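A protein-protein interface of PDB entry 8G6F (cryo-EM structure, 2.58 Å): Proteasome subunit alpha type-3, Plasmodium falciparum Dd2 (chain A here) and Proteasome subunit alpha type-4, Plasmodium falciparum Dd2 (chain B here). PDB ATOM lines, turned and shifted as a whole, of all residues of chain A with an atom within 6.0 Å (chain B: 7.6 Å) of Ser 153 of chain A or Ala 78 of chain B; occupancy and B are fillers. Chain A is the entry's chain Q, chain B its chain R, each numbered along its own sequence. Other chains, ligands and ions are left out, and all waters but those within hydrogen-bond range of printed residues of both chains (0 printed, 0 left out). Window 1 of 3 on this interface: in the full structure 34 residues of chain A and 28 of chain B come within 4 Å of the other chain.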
ATOM      1  N   LEU A  18       2.454 -16.599 -15.975  1.00  0.00           N
ATOM      2  CA  LEU A  18       3.341 -15.974 -15.000  1.00  0.00           C
ATOM      3  C   LEU A  18       2.620 -14.793 -14.362  1.00  0.00           C
ATOM      4  O   LEU A  18       2.326 -13.795 -15.033  1.00  0.00           O
ATOM      5  CB  LEU A  18       4.647 -15.540 -15.660  1.00  0.00           C
ATOM      6  CG  LEU A  18       5.417 -16.664 -16.355  1.00  0.00           C
ATOM      7  CD1 LEU A  18       6.104 -16.154 -17.608  1.00  0.00           C
ATOM      8  CD2 LEU A  18       6.425 -17.280 -15.407  1.00  0.00           C
ATOM      9  N   VAL A  21       4.410 -11.410 -14.693  1.00  0.00           N
ATOM     10  CA  VAL A  21       4.263 -10.806 -16.012  1.00  0.00           C
ATOM     11  C   VAL A  21       2.861 -10.239 -16.188  1.00  0.00           C
ATOM     12  O   VAL A  21       2.681  -9.168 -16.777  1.00  0.00           O
ATOM     13  CB  VAL A  21       4.603 -11.834 -17.105  1.00  0.00           C
ATOM     14  CG1 VAL A  21       4.479 -11.211 -18.473  1.00  0.00           C
ATOM     15  CG2 VAL A  21       5.999 -12.376 -16.895  1.00  0.00           C
ATOM     16  N   LEU A  25       1.931  -6.360 -16.872  1.00  0.00           N
ATOM     17  CA  LEU A  25       1.037  -5.934 -17.944  1.00  0.00           C
ATOM     18  C   LEU A  25      -0.078  -5.046 -17.410  1.00  0.00           C
ATOM     19  O   LEU A  25      -0.495  -4.095 -18.079  1.00  0.00           O
ATOM     20  CB  LEU A  25       0.459  -7.150 -18.662  1.00  0.00           C
ATOM     21  CG  LEU A  25       1.328  -7.683 -19.798  1.00  0.00           C
ATOM     22  CD1 LEU A  25       0.992  -9.128 -20.107  1.00  0.00           C
ATOM     23  CD2 LEU A  25       1.163  -6.819 -21.032  1.00  0.00           C
ATOM     24  N   CYS A 115      14.100  -7.686 -26.361  1.00  0.00           N
ATOM     25  CA  CYS A 115      13.094  -8.652 -25.950  1.00  0.00           C
ATOM     26  C   CYS A 115      13.729  -9.896 -25.350  1.00  0.00           C
ATOM     27  O   CYS A 115      13.149 -10.515 -24.456  1.00  0.00           O
ATOM     28  CB  CYS A 115      12.223  -9.016 -27.147  1.00  0.00           C
ATOM     29  SG  CYS A 115      11.172  -7.674 -27.696  1.00  0.00           S
ATOM     30  N   ASP A 116      14.908 -10.285 -25.834  1.00  0.00           N
ATOM     31  CA  ASP A 116      15.619 -11.404 -25.234  1.00  0.00           C
ATOM     32  C   ASP A 116      16.028 -11.081 -23.809  1.00  0.00           C
ATOM     33  O   ASP A 116      15.969 -11.946 -22.929  1.00  0.00           O
ATOM     34  CB  ASP A 116      16.845 -11.761 -26.071  1.00  0.00           C
ATOM     35  CG  ASP A 116      16.497 -12.573 -27.299  1.00  0.00           C
ATOM     36  OD1 ASP A 116      15.296 -12.779 -27.560  1.00  0.00           O
ATOM     37  OD2 ASP A 116      17.426 -13.009 -28.005  1.00  0.00           O
ATOM     38  N   LYS A 118      14.343  -9.152 -21.805  1.00  0.00           N
ATOM     39  CA  LYS A 118      13.111  -9.264 -21.021  1.00  0.00           C
ATOM     40  C   LYS A 118      12.743 -10.726 -20.762  1.00  0.00           C
ATOM     41  O   LYS A 118      12.374 -11.105 -19.640  1.00  0.00           O
ATOM     42  CB  LYS A 118      11.972  -8.544 -21.735  1.00  0.00           C
ATOM     43  CG  LYS A 118      12.084  -7.039 -21.704  1.00  0.00           C
ATOM     44  CD  LYS A 118      10.754  -6.377 -22.005  1.00  0.00           C
ATOM     45  CE  LYS A 118      10.870  -5.362 -23.124  1.00  0.00           C
ATOM     46  NZ  LYS A 118       9.787  -4.350 -23.060  1.00  0.00           N
ATOM     47  N   GLN A 119      12.829 -11.563 -21.793  1.00  0.00           N
ATOM     48  CA  GLN A 119      12.491 -12.973 -21.634  1.00  0.00           C
ATOM     49  C   GLN A 119      13.426 -13.650 -20.642  1.00  0.00           C
ATOM     50  O   GLN A 119      12.988 -14.460 -19.815  1.00  0.00           O
ATOM     51  CB  GLN A 119      12.548 -13.678 -22.988  1.00  0.00           C
ATOM     52  CG  GLN A 119      11.881 -15.039 -23.014  1.00  0.00           C
ATOM     53  CD  GLN A 119      12.719 -16.128 -22.383  1.00  0.00           C
ATOM     54  OE1 GLN A 119      13.942 -16.048 -22.354  1.00  0.00           O
ATOM     55  NE2 GLN A 119      12.059 -17.155 -21.874  1.00  0.00           N
ATOM     56  N   THR A 122      12.280 -12.964 -17.272  1.00  0.00           N
ATOM     57  CA  THR A 122      11.105 -13.743 -16.882  1.00  0.00           C
ATOM     58  C   THR A 122      11.423 -15.212 -16.630  1.00  0.00           C
ATOM     59  O   THR A 122      10.654 -15.884 -15.937  1.00  0.00           O
ATOM     60  CB  THR A 122      10.009 -13.663 -17.943  1.00  0.00           C
ATOM     61  OG1 THR A 122      10.496 -14.197 -19.178  1.00  0.00           O
ATOM     62  CG2 THR A 122       9.554 -12.233 -18.142  1.00  0.00           C
ATOM     63  N   ASP A 151       6.358  -6.427 -25.178  1.00  0.00           N
ATOM     64  CA  ASP A 151       5.739  -6.473 -23.856  1.00  0.00           C
ATOM     65  C   ASP A 151       6.685  -7.094 -22.829  1.00  0.00           C
ATOM     66  O   ASP A 151       7.765  -7.569 -23.193  1.00  0.00           O
ATOM     67  CB  ASP A 151       4.416  -7.240 -23.924  1.00  0.00           C
ATOM     68  CG  ASP A 151       4.601  -8.737 -23.878  1.00  0.00           C
ATOM     69  OD1 ASP A 151       5.664  -9.223 -24.314  1.00  0.00           O
ATOM     70  OD2 ASP A 151       3.679  -9.435 -23.407  1.00  0.00           O
ATOM     71  N   PRO A 152       6.325  -7.094 -21.540  1.00  0.00           N
ATOM     72  CA  PRO A 152       7.263  -7.586 -20.515  1.00  0.00           C
ATOM     73  C   PRO A 152       7.679  -9.032 -20.685  1.00  0.00           C
ATOM     74  O   PRO A 152       8.766  -9.407 -20.233  1.00  0.00           O
ATOM     75  CB  PRO A 152       6.480  -7.394 -19.211  1.00  0.00           C
ATOM     76  CG  PRO A 152       5.524  -6.345 -19.499  1.00  0.00           C
ATOM     77  CD  PRO A 152       5.125  -6.507 -20.928  1.00  0.00           C
ATOM     78  N   SER A 153       6.843  -9.866 -21.297  1.00  0.00           N
ATOM     79  CA  SER A 153       7.165 -11.279 -21.435  1.00  0.00           C
ATOM     80  C   SER A 153       8.317 -11.527 -22.393  1.00  0.00           C
ATOM     81  O   SER A 153       8.809 -12.656 -22.460  1.00  0.00           O
ATOM     82  CB  SER A 153       5.934 -12.044 -21.915  1.00  0.00           C
ATOM     83  OG  SER A 153       5.439 -11.489 -23.118  1.00  0.00           O
ATOM     84  N   GLY A 154       8.759 -10.510 -23.125  1.00  0.00           N
ATOM     85  CA  GLY A 154       9.671 -10.693 -24.223  1.00  0.00           C
ATOM     86  C   GLY A 154       8.995 -10.889 -25.559  1.00  0.00           C
ATOM     87  O   GLY A 154       9.685 -10.944 -26.581  1.00  0.00           O
ATOM     88  N   ASN A 155       7.672 -11.007 -25.586  1.00  0.00           N
ATOM     89  CA  ASN A 155       6.959 -11.097 -26.847  1.00  0.00           C
ATOM     90  C   ASN A 155       7.000  -9.762 -27.573  1.00  0.00           C
ATOM     91  O   ASN A 155       6.981  -8.690 -26.960  1.00  0.00           O
ATOM     92  CB  ASN A 155       5.505 -11.512 -26.625  1.00  0.00           C
ATOM     93  CG  ASN A 155       5.377 -12.776 -25.812  1.00  0.00           C
ATOM     94  OD1 ASN A 155       4.504 -12.883 -24.954  1.00  0.00           O
ATOM     95  ND2 ASN A 155       6.239 -13.746 -26.079  1.00  0.00           N
ATOM     96  N   PHE B  73       6.241 -24.484 -33.785  1.00  0.00           N
ATOM     97  CA  PHE B  73       6.118 -24.568 -32.338  1.00  0.00           C
ATOM     98  C   PHE B  73       4.760 -24.058 -31.884  1.00  0.00           C
ATOM     99  O   PHE B  73       4.044 -23.375 -32.620  1.00  0.00           O
ATOM    100  CB  PHE B  73       7.237 -23.790 -31.635  1.00  0.00           C
ATOM    101  CG  PHE B  73       7.198 -22.313 -31.881  1.00  0.00           C
ATOM    102  CD1 PHE B  73       6.373 -21.493 -31.132  1.00  0.00           C
ATOM    103  CD2 PHE B  73       7.995 -21.742 -32.852  1.00  0.00           C
ATOM    104  CE1 PHE B  73       6.336 -20.142 -31.358  1.00  0.00           C
ATOM    105  CE2 PHE B  73       7.961 -20.390 -33.079  1.00  0.00           C
ATOM    106  CZ  PHE B  73       7.133 -19.588 -32.328  1.00  0.00           C
ATOM    107  N   GLY B  75       3.023 -22.561 -28.027  1.00  0.00           N
ATOM    108  CA  GLY B  75       3.254 -22.179 -26.648  1.00  0.00           C
ATOM    109  C   GLY B  75       3.568 -20.708 -26.472  1.00  0.00           C
ATOM    110  O   GLY B  75       2.799 -19.848 -26.907  1.00  0.00           O
ATOM    111  N   LEU B  76       4.697 -20.409 -25.835  1.00  0.00           N
ATOM    112  CA  LEU B  76       5.107 -19.041 -25.544  1.00  0.00           C
ATOM    113  C   LEU B  76       6.120 -18.590 -26.588  1.00  0.00           C
ATOM    114  O   LEU B  76       7.159 -19.233 -26.766  1.00  0.00           O
ATOM    115  CB  LEU B  76       5.705 -18.943 -24.142  1.00  0.00           C
ATOM    116  CG  LEU B  76       4.864 -19.517 -23.002  1.00  0.00           C
ATOM    117  CD1 LEU B  76       5.641 -19.479 -21.702  1.00  0.00           C
ATOM    118  CD2 LEU B  76       3.559 -18.765 -22.868  1.00  0.00           C
ATOM    119  N   ASN B  77       5.826 -17.474 -27.258  1.00  0.00           N
ATOM    120  CA  ASN B  77       6.640 -17.053 -28.394  1.00  0.00           C
ATOM    121  C   ASN B  77       8.059 -16.693 -27.973  1.00  0.00           C
ATOM    122  O   ASN B  77       9.015 -16.978 -28.699  1.00  0.00           O
ATOM    123  CB  ASN B  77       5.982 -15.872 -29.101  1.00  0.00           C
ATOM    124  CG  ASN B  77       4.657 -16.235 -29.726  1.00  0.00           C
ATOM    125  OD1 ASN B  77       4.304 -17.410 -29.819  1.00  0.00           O
ATOM    126  ND2 ASN B  77       3.910 -15.228 -30.158  1.00  0.00           N
ATOM    127  N   ALA B  78       8.222 -16.046 -26.819  1.00  0.00           N
ATOM    128  CA  ALA B  78       9.558 -15.636 -26.399  1.00  0.00           C
ATOM    129  C   ALA B  78      10.420 -16.843 -26.045  1.00  0.00           C
ATOM    130  O   ALA B  78      11.600 -16.912 -26.426  1.00  0.00           O
ATOM    131  CB  ALA B  78       9.456 -14.675 -25.218  1.00  0.00           C
ATOM    132  N   ASP B  79       9.846 -17.809 -25.324  1.00  0.00           N
ATOM    133  CA  ASP B  79      10.553 -19.057 -25.064  1.00  0.00           C
ATOM    134  C   ASP B  79      10.899 -19.760 -26.366  1.00  0.00           C
ATOM    135  O   ASP B  79      12.002 -20.298 -26.519  1.00  0.00           O
ATOM    136  CB  ASP B  79       9.700 -19.969 -24.184  1.00  0.00           C
ATOM    137  CG  ASP B  79       9.570 -19.462 -22.765  1.00  0.00           C
ATOM    138  OD1 ASP B  79       9.463 -18.233 -22.575  1.00  0.00           O
ATOM    139  OD2 ASP B  79       9.564 -20.294 -21.835  1.00  0.00           O
ATOM    140  N   ALA B  80       9.963 -19.768 -27.317  1.00  0.00           N
ATOM    141  CA  ALA B  80      10.229 -20.378 -28.612  1.00  0.00           C
ATOM    142  C   ALA B  80      11.407 -19.709 -29.296  1.00  0.00           C
ATOM    143  O   ALA B  80      12.265 -20.384 -29.868  1.00  0.00           O
ATOM    144  CB  ALA B  80       8.993 -20.280 -29.497  1.00  0.00           C
ATOM    145  N   ARG B  81      11.456 -18.380 -29.257  1.00  0.00           N
ATOM    146  CA  ARG B  81      12.537 -17.651 -29.909  1.00  0.00           C
ATOM    147  C   ARG B  81      13.880 -18.004 -29.289  1.00  0.00           C
ATOM    148  O   ARG B  81      14.858 -18.269 -29.999  1.00  0.00           O
ATOM    149  CB  ARG B  81      12.271 -16.151 -29.811  1.00  0.00           C
ATOM    150  CG  ARG B  81      13.272 -15.287 -30.544  1.00  0.00           C
ATOM    151  CD  ARG B  81      12.879 -13.825 -30.486  1.00  0.00           C
ATOM    152  NE  ARG B  81      12.965 -13.288 -29.132  1.00  0.00           N
ATOM    153  CZ  ARG B  81      11.936 -12.873 -28.405  1.00  0.00           C
ATOM    154  NH1 ARG B  81      10.696 -12.915 -28.865  1.00  0.00           N
ATOM    155  NH2 ARG B  81      12.157 -12.405 -27.182  1.00  0.00           N
ATOM    156  N   VAL B  82      13.945 -18.017 -27.959  1.00  0.00           N
ATOM    157  CA  VAL B  82      15.207 -18.331 -27.295  1.00  0.00           C
ATOM    158  C   VAL B  82      15.646 -19.754 -27.624  1.00  0.00           C
ATOM    159  O   VAL B  82      16.817 -20.006 -27.950  1.00  0.00           O
ATOM    160  CB  VAL B  82      15.073 -18.107 -25.779  1.00  0.00           C
ATOM    161  CG1 VAL B  82      16.209 -18.778 -25.036  1.00  0.00           C
ATOM    162  CG2 VAL B  82      15.044 -16.624 -25.481  1.00  0.00           C
ATOM    163  N   LEU B  83      14.712 -20.703 -27.563  1.00  0.00           N
ATOM    164  CA  LEU B  83      15.041 -22.089 -27.869  1.00  0.00           C
ATOM    165  C   LEU B  83      15.504 -22.241 -29.312  1.00  0.00           C
ATOM    166  O   LEU B  83      16.453 -22.980 -29.594  1.00  0.00           O
ATOM    167  CB  LEU B  83      13.824 -22.973 -27.598  1.00  0.00           C
ATOM    168  CG  LEU B  83      14.032 -24.478 -27.453  1.00  0.00           C
ATOM    169  CD1 LEU B  83      15.117 -24.798 -26.444  1.00  0.00           C
ATOM    170  CD2 LEU B  83      12.727 -25.134 -27.061  1.00  0.00           C
ATOM    171  N   VAL B  84      14.846 -21.550 -30.241  1.00  0.00           N
ATOM    172  CA  VAL B  84      15.198 -21.670 -31.649  1.00  0.00           C
ATOM    173  C   VAL B  84      16.581 -21.093 -31.906  1.00  0.00           C
ATOM    174  O   VAL B  84      17.346 -21.625 -32.715  1.00  0.00           O
ATOM    175  CB  VAL B  84      14.125 -20.987 -32.517  1.00  0.00           C
ATOM    176  CG1 VAL B  84      14.671 -20.660 -33.885  1.00  0.00           C
ATOM    177  CG2 VAL B  84      12.908 -21.873 -32.634  1.00  0.00           C
ATOM    178  N   ARG B 125      12.911 -22.170 -14.968  1.00  0.00           N
ATOM    179  CA  ARG B 125      11.613 -22.788 -15.165  1.00  0.00           C
ATOM    180  C   ARG B 125      11.542 -23.458 -16.532  1.00  0.00           C
ATOM    181  O   ARG B 125      12.280 -23.094 -17.453  1.00  0.00           O
ATOM    182  CB  ARG B 125      10.483 -21.759 -15.032  1.00  0.00           C
ATOM    183  CG  ARG B 125      10.459 -20.683 -16.094  1.00  0.00           C
ATOM    184  CD  ARG B 125       9.055 -20.160 -16.301  1.00  0.00           C
ATOM    185  NE  ARG B 125       9.036 -18.983 -17.157  1.00  0.00           N
ATOM    186  CZ  ARG B 125       9.245 -19.002 -18.466  1.00  0.00           C
ATOM    187  NH1 ARG B 125       9.465 -20.132 -19.116  1.00  0.00           N
ATOM    188  NH2 ARG B 125       9.233 -17.857 -19.140  1.00  0.00           N
ATOM    189  N   PHE B 127      10.654 -24.596 -20.323  1.00  0.00           N
ATOM    190  CA  PHE B 127      10.151 -23.966 -21.535  1.00  0.00           C
ATOM    191  C   PHE B 127       8.689 -24.342 -21.737  1.00  0.00           C
ATOM    192  O   PHE B 127       8.337 -25.525 -21.734  1.00  0.00           O
ATOM    193  CB  PHE B 127      10.964 -24.407 -22.749  1.00  0.00           C
ATOM    194  CG  PHE B 127      12.328 -23.791 -22.835  1.00  0.00           C
ATOM    195  CD1 PHE B 127      12.493 -22.508 -23.314  1.00  0.00           C
ATOM    196  CD2 PHE B 127      13.449 -24.506 -22.462  1.00  0.00           C
ATOM    197  CE1 PHE B 127      13.747 -21.944 -23.403  1.00  0.00           C
ATOM    198  CE2 PHE B 127      14.702 -23.946 -22.549  1.00  0.00           C
ATOM    199  CZ  PHE B 127      14.850 -22.664 -23.021  1.00  0.00           C
ATOM    200  N   ILE B 129       6.863 -24.718 -24.311  1.00  0.00           N
ATOM    201  CA  ILE B 129       6.891 -24.830 -25.763  1.00  0.00           C
ATOM    202  C   ILE B 129       6.875 -26.298 -26.166  1.00  0.00           C
ATOM    203  O   ILE B 129       7.544 -27.133 -25.550  1.00  0.00           O
ATOM    204  CB  ILE B 129       8.130 -24.116 -26.345  1.00  0.00           C
ATOM    205  CG1 ILE B 129       7.834 -22.632 -26.540  1.00  0.00           C
ATOM    206  CG2 ILE B 129       8.556 -24.737 -27.660  1.00  0.00           C
ATOM    207  CD1 ILE B 129       6.936 -22.341 -27.718  1.00  0.00           C
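Among the printed residues, pairs that only touch across the chains: Leu 18 of chain A with Arg 125 of chain B (3.6 Å), Gln 119 of chain A with Ala 78 of chain B (3.3 Å), Gln 119 of chain A with Val 82 of chain B (3.4 Å), Gln 119 of chain A with Arg 125 of chain B (3.99 Å), Thr 122 of chain A with Arg 125 of chain B (3.7 Å), Ser 153 of chain A with Ala 78 of chain B (3.5 Å), Gly 154 of chain A with Ala 78 of chain B (3.8 Å) and Asn 155 of chain A with Asn 77 of chain B (3.7 Å).
SG of Cys 115 of chain A lies close to O of Gly 154 of chain A (3.8 Å).
O of Gln 119 of chain A lies within hydrogen-bond range of OG1 of Thr 122 of chain A.
The side-chain carboxylate (OD1) of Asp 151 of chain A is in hydrogen-bond range of the side-chain hydroxyl (OG) of Ser 153 of chain A (2.6 Å).
OD1 of Asp 151 of chain A sits at hydrogen-bond distance from N of Asn 155 of chain A (3.0 Å).
OD1 of Asn 155 of chain A sits at hydrogen-bond distance from OG of Ser 153 of chain A (2.5 Å).
The guanidinium group of Arg 125 of chain B lies within salt-bridge range of the side-chain carboxylate of Asp 79 of chain B, 2.7 Å away.
Of the 14 printed residues of chain B, 6 touch a printed residue of chain A.
Among the printed residues, 13 pairs touch across the chains.
Of the printed residues of chain B, Leu 18 of chain A touches Arg 125.
Of the printed residues of chain B, Cys 115 of chain A touches Arg 81.
Of the printed residues of chain B, Asp 116 of chain A touches Arg 81.
Lys 118 of chain A touches none of the printed residues of chain B.
Printed residues of chain B within 4 Å of Gln 119 of chain A: Ala 78, Asp 79, Val 82 and Arg 125.
Printed residues of chain B within 4 Å of Ser 153 of chain A: Ala 78 (3.5 Å).
Ala 78 of chain B touches just these residues of chain A: Gln 119, Ser 153, Gly 154 and Asn 155.
Leu 83 of chain B touches none of the printed residues of chain A.
The nearest residue of chain B that does not touch Ser 153 of chain A is Asp 79 of chain B (5.6 Å).
The nearest residue of chain A that does not touch Ala 78 of chain B is Cys 115 of chain A (5.6 Å).
The nearest printed residue of chain B that does not touch Gly 154 of chain A is Asn 77 of chain B (6.1 Å).
The backbone carbonyl oxygen of Cys 115 of chain A lies close to the guanidinium group of Arg 81 of chain B.
The guanidinium group of Arg 81 of chain B is in salt-bridge range of the side-chain carboxylate of Asp 116 of chain A, 2.9 Å away.
The side-chain amide nitrogen (NE2) of Gln 119 of chain A lies within hydrogen-bond range of the side-chain carboxylate (OD1) of Asp 79 of chain B, at 2.9 Å.
O of Gly 154 of chain A sits at hydrogen-bond distance from NH2 of Arg 81 of chain B, at 2.9 Å.
N of Ala 78 of chain B lies close to ND2 of Asn 155 of chain A (3.1 Å).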
